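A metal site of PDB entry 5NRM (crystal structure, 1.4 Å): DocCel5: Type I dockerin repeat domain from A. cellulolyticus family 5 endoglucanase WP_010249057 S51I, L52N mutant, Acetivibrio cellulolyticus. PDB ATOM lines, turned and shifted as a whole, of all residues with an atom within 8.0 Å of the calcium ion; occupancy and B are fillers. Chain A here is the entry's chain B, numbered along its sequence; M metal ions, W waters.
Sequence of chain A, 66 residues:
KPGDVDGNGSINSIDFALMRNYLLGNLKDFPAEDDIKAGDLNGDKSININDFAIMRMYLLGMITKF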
ATOM      1  N   MET A  19      17.356   4.596  22.700  1.00  0.00           N
ATOM      2  CA  MET A  19      17.542   6.012  22.396  1.00  0.00           C
ATOM      3  C   MET A  19      17.773   6.225  20.871  1.00  0.00           C
ATOM      4  O   MET A  19      17.296   7.175  20.278  1.00  0.00           O
ATOM      5  CB  MET A  19      18.718   6.534  23.116  1.00  0.00           C
ATOM      6  CG  MET A  19      18.498   6.584  24.598  1.00  0.00           C
ATOM      7  SD  MET A  19      19.912   7.343  25.404  1.00  0.00           S
ATOM      8  CE  MET A  19      19.664   9.047  24.796  1.00  0.00           C
ATOM      9  N   ILE A  36      11.437  11.943  29.763  1.00  0.00           N
ATOM     10  CA  ILE A  36      12.419  13.030  29.883  1.00  0.00           C
ATOM     11  C   ILE A  36      13.453  12.822  30.990  1.00  0.00           C
ATOM     12  O   ILE A  36      14.672  12.964  30.725  1.00  0.00           O
ATOM     13  CB  ILE A  36      11.748  14.424  30.023  1.00  0.00           C
ATOM     14  CG1 ILE A  36      10.694  14.642  28.926  1.00  0.00           C
ATOM     15  CG2 ILE A  36      12.741  15.575  29.907  1.00  0.00           C
ATOM     16  CD1 ILE A  36      11.132  14.511  27.464  1.00  0.00           C
ATOM     17  N   GLY A  39      15.648  10.037  29.558  1.00  0.00           N
ATOM     18  CA  GLY A  39      16.313  10.220  28.234  1.00  0.00           C
ATOM     19  C   GLY A  39      17.109  11.543  28.008  1.00  0.00           C
ATOM     20  O   GLY A  39      17.948  11.641  27.106  1.00  0.00           O
ATOM     21  N   ASP A  40      16.750  12.559  28.754  1.00  0.00           N
ATOM     22  CA  ASP A  40      17.438  13.844  28.611  1.00  0.00           C
ATOM     23  C   ASP A  40      18.619  13.986  29.537  1.00  0.00           C
ATOM     24  O   ASP A  40      18.445  14.151  30.740  1.00  0.00           O
ATOM     25  CB  ASP A  40      16.496  14.990  28.841  1.00  0.00           C
ATOM     26  CG  ASP A  40      17.195  16.363  28.630  1.00  0.00           C
ATOM     27  OD1 ASP A  40      18.008  16.606  27.599  1.00  0.00           O
ATOM     28  OD2 ASP A  40      16.775  17.193  29.485  1.00  0.00           O
ATOM     29  N   LEU A  41      19.789  13.989  28.919  1.00  0.00           N
ATOM     30  CA  LEU A  41      21.071  13.890  29.626  1.00  0.00           C
ATOM     31  C   LEU A  41      21.810  15.188  29.615  1.00  0.00           C
ATOM     32  O   LEU A  41      22.844  15.294  30.318  1.00  0.00           O
ATOM     33  CB  LEU A  41      21.907  12.773  29.009  1.00  0.00           C
ATOM     34  CG  LEU A  41      21.224  11.401  29.048  1.00  0.00           C
ATOM     35  CD1 LEU A  41      22.061  10.299  28.478  1.00  0.00           C
ATOM     36  CD2 LEU A  41      20.728  11.068  30.461  1.00  0.00           C
ATOM     37  N   ASN A  42      21.330  16.200  28.860  1.00  0.00           N
ATOM     38  CA  ASN A  42      21.993  17.518  28.865  1.00  0.00           C
ATOM     39  C   ASN A  42      21.109  18.637  29.344  1.00  0.00           C
ATOM     40  O   ASN A  42      21.514  19.816  29.343  1.00  0.00           O
ATOM     41  CB  ASN A  42      22.561  17.874  27.482  1.00  0.00           C
ATOM     42  CG  ASN A  42      21.498  17.880  26.411  1.00  0.00           C
ATOM     43  OD1 ASN A  42      20.320  17.784  26.704  1.00  0.00           O
ATOM     44  ND2 ASN A  42      21.930  18.048  25.147  1.00  0.00           N
ATOM     45  N   GLY A  43      19.843  18.340  29.673  1.00  0.00           N
ATOM     46  CA  GLY A  43      19.050  19.280  30.437  1.00  0.00           C
ATOM     47  C   GLY A  43      18.259  20.330  29.631  1.00  0.00           C
ATOM     48  O   GLY A  43      17.877  21.353  30.160  1.00  0.00           O
ATOM     49  N   ASP A  44      18.027  20.079  28.350  1.00  0.00           N
ATOM     50  CA  ASP A  44      17.068  20.903  27.555  1.00  0.00           C
ATOM     51  C   ASP A  44      15.654  20.335  27.516  1.00  0.00           C
ATOM     52  O   ASP A  44      14.856  20.760  26.687  1.00  0.00           O
ATOM     53  CB  ASP A  44      17.558  21.161  26.123  1.00  0.00           C
ATOM     54  CG  ASP A  44      17.884  19.861  25.338  1.00  0.00           C
ATOM     55  OD1 ASP A  44      17.595  18.700  25.779  1.00  0.00           O
ATOM     56  OD2 ASP A  44      18.638  19.989  24.323  1.00  0.00           O
ATOM     57  N   LYS A  45      15.370  19.333  28.364  1.00  0.00           N
ATOM     58  CA  LYS A  45      14.054  18.665  28.373  1.00  0.00           C
ATOM     59  C   LYS A  45      13.606  18.103  27.012  1.00  0.00           C
ATOM     60  O   LYS A  45      12.420  17.991  26.747  1.00  0.00           O
ATOM     61  CB  LYS A  45      13.012  19.525  28.986  1.00  0.00           C
ATOM     62  CG  LYS A  45      13.491  20.057  30.309  1.00  0.00           C
ATOM     63  CD  LYS A  45      12.342  20.468  31.135  1.00  0.00           C
ATOM     64  CE  LYS A  45      12.787  21.029  32.449  1.00  0.00           C
ATOM     65  NZ  LYS A  45      11.696  21.912  32.930  1.00  0.00           N
ATOM     66  N   SER A  46      14.569  17.751  26.152  1.00  0.00           N
ATOM     67  CA  SER A  46      14.278  17.103  24.887  1.00  0.00           C
ATOM     68  C   SER A  46      15.251  15.950  24.706  1.00  0.00           C
ATOM     69  O   SER A  46      16.318  15.925  25.318  1.00  0.00           O
ATOM     70  CB  SER A  46      14.307  18.102  23.708  1.00  0.00           C
ATOM     71  OG  SER A  46      15.629  18.505  23.373  1.00  0.00           O
ATOM     72  N   ILE A  47      14.860  14.988  23.892  1.00  0.00           N
ATOM     73  CA  ILE A  47      15.741  13.892  23.518  1.00  0.00           C
ATOM     74  C   ILE A  47      16.209  13.978  22.065  1.00  0.00           C
ATOM     75  O   ILE A  47      15.422  14.041  21.102  1.00  0.00           O
ATOM     76  CB  ILE A  47      15.050  12.543  23.811  1.00  0.00           C
ATOM     77  CG1 ILE A  47      14.693  12.417  25.297  1.00  0.00           C
ATOM     78  CG2 ILE A  47      15.910  11.397  23.324  1.00  0.00           C
ATOM     79  CD1 ILE A  47      13.344  11.788  25.483  1.00  0.00           C
ATOM     80  N   ASN A  48      17.518  14.120  21.872  1.00  0.00           N
ATOM     81  CA  ASN A  48      18.005  14.270  20.515  1.00  0.00           C
ATOM     82  C   ASN A  48      19.407  13.636  20.411  1.00  0.00           C
ATOM     83  O   ASN A  48      19.859  12.939  21.334  1.00  0.00           O
ATOM     84  CB  ASN A  48      17.921  15.731  20.054  1.00  0.00           C
ATOM     85  CG  ASN A  48      19.104  16.548  20.474  1.00  0.00           C
ATOM     86  OD1 ASN A  48      19.724  16.216  21.456  1.00  0.00           O
ATOM     87  ND2 ASN A  48      19.413  17.616  19.733  1.00  0.00           N
ATOM     88  N   ILE A  49      20.050  13.817  19.248  1.00  0.00           N
ATOM     89  CA  ILE A  49      21.354  13.159  18.990  1.00  0.00           C
ATOM     90  C   ILE A  49      22.375  13.506  20.100  1.00  0.00           C
ATOM     91  O   ILE A  49      23.275  12.713  20.408  1.00  0.00           O
ATOM     92  CB  ILE A  49      21.871  13.524  17.544  1.00  0.00           C
ATOM     93  CG1 ILE A  49      23.041  12.594  17.099  1.00  0.00           C
ATOM     94  CG2 ILE A  49      22.332  14.962  17.475  1.00  0.00           C
ATOM     95  CD1 ILE A  49      22.617  11.195  16.708  1.00  0.00           C
ATOM     96  N   ASN A  50      22.265  14.686  20.707  1.00  0.00           N
ATOM     97  CA  ASN A  50      23.229  15.041  21.725  1.00  0.00           C
ATOM     98  C   ASN A  50      23.113  14.147  22.995  1.00  0.00           C
ATOM     99  O   ASN A  50      24.119  13.803  23.606  1.00  0.00           O
ATOM    100  CB  ASN A  50      23.198  16.546  21.988  1.00  0.00           C
ATOM    101  CG  ASN A  50      23.373  17.358  20.688  1.00  0.00           C
ATOM    102  OD1 ASN A  50      22.650  17.210  19.693  1.00  0.00           O
ATOM    103  ND2 ASN A  50      24.333  18.228  20.712  1.00  0.00           N
ATOM    104  N   ASP A  51      21.906  13.800  23.405  1.00  0.00           N
ATOM    105  CA  ASP A  51      21.717  12.902  24.570  1.00  0.00           C
ATOM    106  C   ASP A  51      22.296  11.550  24.271  1.00  0.00           C
ATOM    107  O   ASP A  51      22.851  10.890  25.163  1.00  0.00           O
ATOM    108  CB  ASP A  51      20.229  12.773  24.886  1.00  0.00           C
ATOM    109  CG  ASP A  51      19.597  14.120  25.174  1.00  0.00           C
ATOM    110  OD1 ASP A  51      19.886  14.686  26.248  1.00  0.00           O
ATOM    111  OD2 ASP A  51      18.819  14.621  24.307  1.00  0.00           O
ATOM    112  N   PHE A  52      22.098  11.112  23.038  1.00  0.00           N
ATOM    113  CA  PHE A  52      22.670   9.828  22.553  1.00  0.00           C
ATOM    114  C   PHE A  52      24.201   9.885  22.582  1.00  0.00           C
ATOM    115  O   PHE A  52      24.842   8.964  23.104  1.00  0.00           O
ATOM    116  CB  PHE A  52      22.150   9.611  21.119  1.00  0.00           C
ATOM    117  CG  PHE A  52      22.700   8.429  20.395  1.00  0.00           C
ATOM    118  CD1 PHE A  52      22.218   7.162  20.632  1.00  0.00           C
ATOM    119  CD2 PHE A  52      23.690   8.589  19.431  1.00  0.00           C
ATOM    120  CE1 PHE A  52      22.745   6.054  19.936  1.00  0.00           C
ATOM    121  CE2 PHE A  52      24.214   7.502  18.758  1.00  0.00           C
ATOM    122  CZ  PHE A  52      23.710   6.231  18.975  1.00  0.00           C
ATOM    123  N   ILE A  54      26.016  11.664  24.540  1.00  0.00           N
ATOM    124  CA  ILE A  54      26.371  11.633  25.963  1.00  0.00           C
ATOM    125  C   ILE A  54      26.279  10.213  26.542  1.00  0.00           C
ATOM    126  O   ILE A  54      27.170   9.816  27.339  1.00  0.00           O
ATOM    127  CB  ILE A  54      25.549  12.647  26.806  1.00  0.00           C
ATOM    128  CG1 ILE A  54      25.940  14.088  26.538  1.00  0.00           C
ATOM    129  CG2 ILE A  54      25.608  12.405  28.311  1.00  0.00           C
ATOM    130  CD1 ILE A  54      24.933  15.128  27.040  1.00  0.00           C
HETATM  131 CA    CA M   1      18.548  16.622  25.584  1.00  0.00          CA
HETATM  132  O   HOH W   1      19.483  17.551  23.414  1.00  0.00           O
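OD2 of Asp 40 lies close to N of Gly 43, 3.3 Å away.
The side-chain carboxylate of Asp 40 is in hydrogen-bond range of the backbone NH of Lys 45, 2.8 Å away.
The side-chain carboxylate of Asp 51 lies close to the backbone NH of Asn 48 (2.8 Å).
The backbone NH (N) of Leu 41 lies close to the side-chain carboxylate (OD1) of Asp 51 (2.8 Å).
The calcium ion is bound by OD1 of Asp 40 (2.1 Å), OD1 of Asp 44 (2.3 Å), O of Ser 46 (2.4 Å), OD2 of Asp 51 (2.4 Å), OD1 of Asn 42 (2.4 Å), OD1 of Asp 51 (2.4 Å) and water W1 (2.5 Å).
Water W1 lies within hydrogen-bond range of OD2 of Asp 44 (2.7 Å) and ND2 of Asn 42 (3.0 Å).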
